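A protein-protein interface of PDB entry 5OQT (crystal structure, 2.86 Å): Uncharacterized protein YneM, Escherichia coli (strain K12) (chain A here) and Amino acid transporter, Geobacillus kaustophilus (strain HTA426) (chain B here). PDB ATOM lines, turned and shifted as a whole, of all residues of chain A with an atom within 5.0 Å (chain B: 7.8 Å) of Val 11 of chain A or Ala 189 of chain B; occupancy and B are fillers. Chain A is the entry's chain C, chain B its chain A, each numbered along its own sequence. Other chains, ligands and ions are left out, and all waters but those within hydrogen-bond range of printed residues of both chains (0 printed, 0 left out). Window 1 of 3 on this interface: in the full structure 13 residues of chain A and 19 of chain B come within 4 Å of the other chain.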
ATOM      1  N   VAL A   7      -5.727   9.202  25.489  1.00  0.00           N
ATOM      2  CA  VAL A   7      -4.484   8.537  25.911  1.00  0.00           C
ATOM      3  C   VAL A   7      -3.557   8.337  24.695  1.00  0.00           C
ATOM      4  O   VAL A   7      -2.370   8.666  24.775  1.00  0.00           O
ATOM      5  CB  VAL A   7      -4.764   7.237  26.726  1.00  0.00           C
ATOM      6  CG1 VAL A   7      -3.649   6.205  26.596  1.00  0.00           C
ATOM      7  CG2 VAL A   7      -5.016   7.558  28.191  1.00  0.00           C
ATOM      8  N   PHE A   8      -4.122   7.874  23.564  1.00  0.00           N
ATOM      9  CA  PHE A   8      -3.405   7.683  22.305  1.00  0.00           C
ATOM     10  C   PHE A   8      -2.819   9.026  21.809  1.00  0.00           C
ATOM     11  O   PHE A   8      -1.604   9.140  21.611  1.00  0.00           O
ATOM     12  CB  PHE A   8      -4.348   7.059  21.250  1.00  0.00           C
ATOM     13  CG  PHE A   8      -3.827   7.018  19.829  1.00  0.00           C
ATOM     14  CD1 PHE A   8      -2.940   6.028  19.425  1.00  0.00           C
ATOM     15  CD2 PHE A   8      -4.254   7.948  18.886  1.00  0.00           C
ATOM     16  CE1 PHE A   8      -2.455   5.994  18.118  1.00  0.00           C
ATOM     17  CE2 PHE A   8      -3.770   7.911  17.577  1.00  0.00           C
ATOM     18  CZ  PHE A   8      -2.867   6.941  17.206  1.00  0.00           C
ATOM     19  N   MET A   9      -3.695  10.035  21.638  1.00  0.00           N
ATOM     20  CA  MET A   9      -3.355  11.376  21.174  1.00  0.00           C
ATOM     21  C   MET A   9      -2.280  12.060  22.010  1.00  0.00           C
ATOM     22  O   MET A   9      -1.378  12.679  21.445  1.00  0.00           O
ATOM     23  CB  MET A   9      -4.616  12.240  21.110  1.00  0.00           C
ATOM     24  CG  MET A   9      -5.373  12.087  19.831  1.00  0.00           C
ATOM     25  SD  MET A   9      -4.425  12.788  18.467  1.00  0.00           S
ATOM     26  CE  MET A   9      -5.631  13.957  17.811  1.00  0.00           C
ATOM     27  N   ALA A  10      -2.358  11.917  23.344  1.00  0.00           N
ATOM     28  CA  ALA A  10      -1.406  12.512  24.276  1.00  0.00           C
ATOM     29  C   ALA A  10       0.002  11.950  24.139  1.00  0.00           C
ATOM     30  O   ALA A  10       0.955  12.730  24.137  1.00  0.00           O
ATOM     31  CB  ALA A  10      -1.893  12.352  25.700  1.00  0.00           C
ATOM     32  N   VAL A  11       0.146  10.614  24.010  1.00  0.00           N
ATOM     33  CA  VAL A  11       1.482  10.018  23.898  1.00  0.00           C
ATOM     34  C   VAL A  11       2.117  10.313  22.529  1.00  0.00           C
ATOM     35  O   VAL A  11       3.330  10.522  22.484  1.00  0.00           O
ATOM     36  CB  VAL A  11       1.578   8.534  24.296  1.00  0.00           C
ATOM     37  CG1 VAL A  11       1.285   8.354  25.780  1.00  0.00           C
ATOM     38  CG2 VAL A  11       0.653   7.674  23.468  1.00  0.00           C
ATOM     39  N   LEU A  12       1.313  10.424  21.441  1.00  0.00           N
ATOM     40  CA  LEU A  12       1.882  10.808  20.145  1.00  0.00           C
ATOM     41  C   LEU A  12       2.593  12.148  20.351  1.00  0.00           C
ATOM     42  O   LEU A  12       3.778  12.243  20.052  1.00  0.00           O
ATOM     43  CB  LEU A  12       0.836  10.989  19.023  1.00  0.00           C
ATOM     44  CG  LEU A  12      -0.087   9.853  18.616  1.00  0.00           C
ATOM     45  CD1 LEU A  12      -1.017  10.336  17.547  1.00  0.00           C
ATOM     46  CD2 LEU A  12       0.678   8.641  18.092  1.00  0.00           C
ATOM     47  N   GLY A  13       1.872  13.123  20.929  1.00  0.00           N
ATOM     48  CA  GLY A  13       2.348  14.470  21.224  1.00  0.00           C
ATOM     49  C   GLY A  13       3.558  14.538  22.135  1.00  0.00           C
ATOM     50  O   GLY A  13       4.425  15.385  21.926  1.00  0.00           O
ATOM     51  N   ILE A  14       3.630  13.643  23.145  1.00  0.00           N
ATOM     52  CA  ILE A  14       4.752  13.568  24.093  1.00  0.00           C
ATOM     53  C   ILE A  14       6.021  13.111  23.359  1.00  0.00           C
ATOM     54  O   ILE A  14       7.058  13.764  23.487  1.00  0.00           O
ATOM     55  CB  ILE A  14       4.392  12.705  25.337  1.00  0.00           C
ATOM     56  CG1 ILE A  14       3.491  13.506  26.309  1.00  0.00           C
ATOM     57  CG2 ILE A  14       5.639  12.196  26.055  1.00  0.00           C
ATOM     58  CD1 ILE A  14       2.462  12.667  27.143  1.00  0.00           C
ATOM     59  N   ILE A  15       5.910  12.032  22.558  1.00  0.00           N
ATOM     60  CA  ILE A  15       6.988  11.469  21.739  1.00  0.00           C
ATOM     61  C   ILE A  15       7.372  12.458  20.601  1.00  0.00           C
ATOM     62  O   ILE A  15       8.558  12.652  20.342  1.00  0.00           O
ATOM     63  CB  ILE A  15       6.597  10.056  21.220  1.00  0.00           C
ATOM     64  CG1 ILE A  15       6.437   9.066  22.379  1.00  0.00           C
ATOM     65  CG2 ILE A  15       7.602   9.528  20.200  1.00  0.00           C
ATOM     66  CD1 ILE A  15       5.463   7.948  22.106  1.00  0.00           C
ATOM     67  N   LEU A  16       6.383  13.090  19.946  1.00  0.00           N
ATOM     68  CA  LEU A  16       6.658  14.070  18.897  1.00  0.00           C
ATOM     69  C   LEU A  16       7.269  15.347  19.473  1.00  0.00           C
ATOM     70  O   LEU A  16       7.982  16.046  18.761  1.00  0.00           O
ATOM     71  CB  LEU A  16       5.434  14.386  18.026  1.00  0.00           C
ATOM     72  CG  LEU A  16       4.953  13.278  17.099  1.00  0.00           C
ATOM     73  CD1 LEU A  16       3.519  13.528  16.670  1.00  0.00           C
ATOM     74  CD2 LEU A  16       5.855  13.116  15.891  1.00  0.00           C
ATOM     75  N   PHE B  30     -12.669   2.653  17.461  1.00  0.00           N
ATOM     76  CA  PHE B  30     -11.321   3.142  17.750  1.00  0.00           C
ATOM     77  C   PHE B  30     -10.433   2.036  18.342  1.00  0.00           C
ATOM     78  O   PHE B  30      -9.293   1.853  17.881  1.00  0.00           O
ATOM     79  CB  PHE B  30     -11.343   4.380  18.676  1.00  0.00           C
ATOM     80  CG  PHE B  30      -9.961   4.831  19.108  1.00  0.00           C
ATOM     81  CD1 PHE B  30      -9.446   4.462  20.348  1.00  0.00           C
ATOM     82  CD2 PHE B  30      -9.146   5.565  18.246  1.00  0.00           C
ATOM     83  CE1 PHE B  30      -8.150   4.832  20.721  1.00  0.00           C
ATOM     84  CE2 PHE B  30      -7.859   5.958  18.633  1.00  0.00           C
ATOM     85  CZ  PHE B  30      -7.365   5.577  19.860  1.00  0.00           C
ATOM     86  N   MET B  34      -6.880   0.156  16.828  1.00  0.00           N
ATOM     87  CA  MET B  34      -5.670   0.004  17.649  1.00  0.00           C
ATOM     88  C   MET B  34      -5.240  -1.449  17.641  1.00  0.00           C
ATOM     89  O   MET B  34      -4.057  -1.730  17.474  1.00  0.00           O
ATOM     90  CB  MET B  34      -5.929   0.458  19.097  1.00  0.00           C
ATOM     91  CG  MET B  34      -6.277   1.916  19.231  1.00  0.00           C
ATOM     92  SD  MET B  34      -4.906   3.007  18.785  1.00  0.00           S
ATOM     93  CE  MET B  34      -5.475   3.624  17.201  1.00  0.00           C
ATOM     94  N   ILE B  37      -3.888  -2.002  14.060  1.00  0.00           N
ATOM     95  CA  ILE B  37      -2.570  -1.350  13.863  1.00  0.00           C
ATOM     96  C   ILE B  37      -1.476  -2.078  14.664  1.00  0.00           C
ATOM     97  O   ILE B  37      -0.387  -2.320  14.138  1.00  0.00           O
ATOM     98  CB  ILE B  37      -2.584   0.195  14.106  1.00  0.00           C
ATOM     99  CG1 ILE B  37      -3.422   0.925  13.034  1.00  0.00           C
ATOM    100  CG2 ILE B  37      -1.160   0.765  14.115  1.00  0.00           C
ATOM    101  CD1 ILE B  37      -3.984   2.246  13.460  1.00  0.00           C
ATOM    102  N   PHE B 183      -4.014   0.146  27.770  1.00  0.00           N
ATOM    103  CA  PHE B 183      -2.610  -0.205  27.654  1.00  0.00           C
ATOM    104  C   PHE B 183      -2.242  -0.447  26.198  1.00  0.00           C
ATOM    105  O   PHE B 183      -1.147  -0.070  25.796  1.00  0.00           O
ATOM    106  CB  PHE B 183      -2.240  -1.395  28.547  1.00  0.00           C
ATOM    107  CG  PHE B 183      -0.748  -1.574  28.696  1.00  0.00           C
ATOM    108  CD1 PHE B 183       0.002  -0.689  29.464  1.00  0.00           C
ATOM    109  CD2 PHE B 183      -0.088  -2.610  28.049  1.00  0.00           C
ATOM    110  CE1 PHE B 183       1.392  -0.837  29.574  1.00  0.00           C
ATOM    111  CE2 PHE B 183       1.300  -2.764  28.172  1.00  0.00           C
ATOM    112  CZ  PHE B 183       2.029  -1.877  28.929  1.00  0.00           C
ATOM    113  N   ASN B 184      -3.173  -0.995  25.394  1.00  0.00           N
ATOM    114  CA  ASN B 184      -2.954  -1.204  23.964  1.00  0.00           C
ATOM    115  C   ASN B 184      -2.931   0.123  23.193  1.00  0.00           C
ATOM    116  O   ASN B 184      -2.203   0.225  22.210  1.00  0.00           O
ATOM    117  CB  ASN B 184      -3.979  -2.165  23.365  1.00  0.00           C
ATOM    118  CG  ASN B 184      -3.633  -2.635  21.965  1.00  0.00           C
ATOM    119  OD1 ASN B 184      -2.510  -3.083  21.673  1.00  0.00           O
ATOM    120  ND2 ASN B 184      -4.599  -2.535  21.062  1.00  0.00           N
ATOM    121  N   ALA B 185      -3.697   1.141  23.646  1.00  0.00           N
ATOM    122  CA  ALA B 185      -3.716   2.470  23.023  1.00  0.00           C
ATOM    123  C   ALA B 185      -2.377   3.180  23.271  1.00  0.00           C
ATOM    124  O   ALA B 185      -1.930   3.942  22.411  1.00  0.00           O
ATOM    125  CB  ALA B 185      -4.863   3.303  23.571  1.00  0.00           C
ATOM    126  N   VAL B 186      -1.723   2.896  24.430  1.00  0.00           N
ATOM    127  CA  VAL B 186      -0.409   3.436  24.798  1.00  0.00           C
ATOM    128  C   VAL B 186       0.651   2.916  23.820  1.00  0.00           C
ATOM    129  O   VAL B 186       1.271   3.737  23.148  1.00  0.00           O
ATOM    130  CB  VAL B 186       0.008   3.141  26.266  1.00  0.00           C
ATOM    131  CG1 VAL B 186       1.361   3.772  26.594  1.00  0.00           C
ATOM    132  CG2 VAL B 186      -1.053   3.597  27.258  1.00  0.00           C
ATOM    133  N   ILE B 187       0.854   1.570  23.744  1.00  0.00           N
ATOM    134  CA  ILE B 187       1.866   0.919  22.885  1.00  0.00           C
ATOM    135  C   ILE B 187       1.679   1.230  21.397  1.00  0.00           C
ATOM    136  O   ILE B 187       2.675   1.485  20.710  1.00  0.00           O
ATOM    137  CB  ILE B 187       2.023  -0.616  23.098  1.00  0.00           C
ATOM    138  CG1 ILE B 187       1.805  -1.053  24.545  1.00  0.00           C
ATOM    139  CG2 ILE B 187       3.375  -1.122  22.573  1.00  0.00           C
ATOM    140  CD1 ILE B 187       0.971  -2.288  24.613  1.00  0.00           C
ATOM    141  N   VAL B 188       0.420   1.192  20.898  1.00  0.00           N
ATOM    142  CA  VAL B 188       0.129   1.470  19.487  1.00  0.00           C
ATOM    143  C   VAL B 188       0.526   2.916  19.158  1.00  0.00           C
ATOM    144  O   VAL B 188       1.157   3.147  18.120  1.00  0.00           O
ATOM    145  CB  VAL B 188      -1.307   1.081  19.062  1.00  0.00           C
ATOM    146  CG1 VAL B 188      -1.658   1.625  17.681  1.00  0.00           C
ATOM    147  CG2 VAL B 188      -1.476  -0.434  19.092  1.00  0.00           C
ATOM    148  N   ALA B 189       0.281   3.854  20.089  1.00  0.00           N
ATOM    149  CA  ALA B 189       0.708   5.227  19.891  1.00  0.00           C
ATOM    150  C   ALA B 189       2.230   5.327  19.894  1.00  0.00           C
ATOM    151  O   ALA B 189       2.758   6.104  19.100  1.00  0.00           O
ATOM    152  CB  ALA B 189       0.115   6.123  20.944  1.00  0.00           C
ATOM    153  N   ILE B 190       2.945   4.500  20.712  1.00  0.00           N
ATOM    154  CA  ILE B 190       4.421   4.484  20.733  1.00  0.00           C
ATOM    155  C   ILE B 190       4.926   4.114  19.322  1.00  0.00           C
ATOM    156  O   ILE B 190       5.795   4.782  18.772  1.00  0.00           O
ATOM    157  CB  ILE B 190       5.004   3.540  21.832  1.00  0.00           C
ATOM    158  CG1 ILE B 190       4.572   3.975  23.241  1.00  0.00           C
ATOM    159  CG2 ILE B 190       6.534   3.446  21.733  1.00  0.00           C
ATOM    160  CD1 ILE B 190       4.791   2.944  24.324  1.00  0.00           C
ATOM    161  N   LYS B 191       4.323   3.085  18.733  1.00  0.00           N
ATOM    162  CA  LYS B 191       4.640   2.591  17.404  1.00  0.00           C
ATOM    163  C   LYS B 191       4.303   3.600  16.300  1.00  0.00           C
ATOM    164  O   LYS B 191       5.141   3.828  15.428  1.00  0.00           O
ATOM    165  CB  LYS B 191       3.882   1.295  17.166  1.00  0.00           C
ATOM    166  CG  LYS B 191       4.754   0.182  16.632  1.00  0.00           C
ATOM    167  CD  LYS B 191       3.917  -0.987  16.132  1.00  0.00           C
ATOM    168  CE  LYS B 191       2.825  -1.470  17.057  1.00  0.00           C
ATOM    169  NZ  LYS B 191       2.482  -2.866  16.744  1.00  0.00           N
ATOM    170  N   VAL B 192       3.080   4.182  16.325  1.00  0.00           N
ATOM    171  CA  VAL B 192       2.643   5.167  15.329  1.00  0.00           C
ATOM    172  C   VAL B 192       3.502   6.443  15.411  1.00  0.00           C
ATOM    173  O   VAL B 192       4.033   6.876  14.387  1.00  0.00           O
ATOM    174  CB  VAL B 192       1.121   5.440  15.401  1.00  0.00           C
ATOM    175  CG1 VAL B 192       0.717   6.648  14.553  1.00  0.00           C
ATOM    176  CG2 VAL B 192       0.341   4.208  14.974  1.00  0.00           C
ATOM    177  N   ALA B 193       3.682   6.999  16.624  1.00  0.00           N
ATOM    178  CA  ALA B 193       4.500   8.190  16.822  1.00  0.00           C
ATOM    179  C   ALA B 193       5.958   8.033  16.327  1.00  0.00           C
ATOM    180  O   ALA B 193       6.445   8.960  15.679  1.00  0.00           O
ATOM    181  CB  ALA B 193       4.475   8.616  18.277  1.00  0.00           C
ATOM    182  N   VAL B 194       6.634   6.868  16.592  1.00  0.00           N
ATOM    183  CA  VAL B 194       8.029   6.645  16.171  1.00  0.00           C
ATOM    184  C   VAL B 194       8.150   6.609  14.649  1.00  0.00           C
ATOM    185  O   VAL B 194       9.093   7.189  14.113  1.00  0.00           O
ATOM    186  CB  VAL B 194       8.798   5.468  16.842  1.00  0.00           C
ATOM    187  CG1 VAL B 194       8.834   5.612  18.361  1.00  0.00           C
ATOM    188  CG2 VAL B 194       8.291   4.093  16.413  1.00  0.00           C
ATOM    189  N   VAL B 195       7.178   6.004  13.962  1.00  0.00           N
ATOM    190  CA  VAL B 195       7.131   5.959  12.505  1.00  0.00           C
ATOM    191  C   VAL B 195       7.046   7.409  11.994  1.00  0.00           C
ATOM    192  O   VAL B 195       7.908   7.817  11.199  1.00  0.00           O
ATOM    193  CB  VAL B 195       5.939   5.092  12.014  1.00  0.00           C
ATOM    194  CG1 VAL B 195       5.640   5.326  10.536  1.00  0.00           C
ATOM    195  CG2 VAL B 195       6.177   3.612  12.295  1.00  0.00           C
ATOM    196  N   LEU B 196       6.048   8.196  12.507  1.00  0.00           N
ATOM    197  CA  LEU B 196       5.840   9.608  12.140  1.00  0.00           C
ATOM    198  C   LEU B 196       7.092  10.442  12.399  1.00  0.00           C
ATOM    199  O   LEU B 196       7.421  11.309  11.585  1.00  0.00           O
ATOM    200  CB  LEU B 196       4.615  10.244  12.836  1.00  0.00           C
ATOM    201  CG  LEU B 196       3.205   9.697  12.495  1.00  0.00           C
ATOM    202  CD1 LEU B 196       2.149  10.275  13.443  1.00  0.00           C
ATOM    203  CD2 LEU B 196       2.816   9.960  11.047  1.00  0.00           C
ATOM    204  N   PHE B 305      15.763   6.307  19.965  1.00  0.00           N
ATOM    205  CA  PHE B 305      14.388   6.591  20.344  1.00  0.00           C
ATOM    206  C   PHE B 305      13.399   5.798  19.441  1.00  0.00           C
ATOM    207  O   PHE B 305      12.404   5.262  19.939  1.00  0.00           O
ATOM    208  CB  PHE B 305      14.162   8.110  20.280  1.00  0.00           C
ATOM    209  CG  PHE B 305      13.011   8.632  21.097  1.00  0.00           C
ATOM    210  CD1 PHE B 305      12.015   9.398  20.509  1.00  0.00           C
ATOM    211  CD2 PHE B 305      12.921   8.358  22.459  1.00  0.00           C
ATOM    212  CE1 PHE B 305      10.941   9.880  21.267  1.00  0.00           C
ATOM    213  CE2 PHE B 305      11.835   8.822  23.215  1.00  0.00           C
ATOM    214  CZ  PHE B 305      10.846   9.572  22.612  1.00  0.00           C
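Val 186 of chain B touches Val 7 of chain A. Phe 8 of chain A touches Phe 30 of chain B. SD of Met 34 of chain B touches CD1 of Phe 8 of chain A, at 3.7 Å. O of Ala 185 of chain B touches CD1 of Phe 8 of chain A, at 3.8 Å. CD1 of Phe 8 of chain A touches CB of Ala 189 of chain B (3.4 Å). CG2 of Val 11 of chain A touches O of Val 186 of chain B, at 3.998 Å. Leu 12 of chain A touches Ala 189 of chain B (CD2 to O, 3.4 Å). Ala 193 of chain B touches Leu 12 of chain A (N to CD2, 3.7 Å). CG2 of Ile 15 of chain A touches CB of Ala 193 of chain B, at 3.8 Å. CE1 of Phe 305 of chain B touches CG2 of Ile 15 of chain A, at 3.5 Å.
Printed residues of chain B within 4 Å of Val 11 of chain A: Val 186 and Ala 189. Of the printed residues of chain A, Ile 190 of chain B touches Ile 15. Of the printed residues of chain B, Leu 12 of chain A touches Ala 189 and Ala 193. Of the printed residues of chain A, Phe 305 of chain B touches Ile 15. The nearest residue of chain A that does not touch Ala 189 of chain B is Ile 15 of chain A (4.4 Å). The nearest printed residue of chain A that does not touch Phe 305 of chain B is Ile 14 of chain A (5.7 Å).
Of the 10 printed residues of chain A, 5 touch a printed residue of chain B. Hydrophobic or aromatic side chains of chain A that line the printed part of chain B: Val 7, Phe 8, Val 11, Leu 12 and Ile 15. Along chain A the printed residues that touch a printed residue of chain B span positions 7 to 15. Along chain B the printed residues that touch a printed residue of chain A span positions 30 to 305. Among the printed residues, no Asp or Glu carboxylate lies within 4 Å of a Lys or Arg side-chain nitrogen of the other chain.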
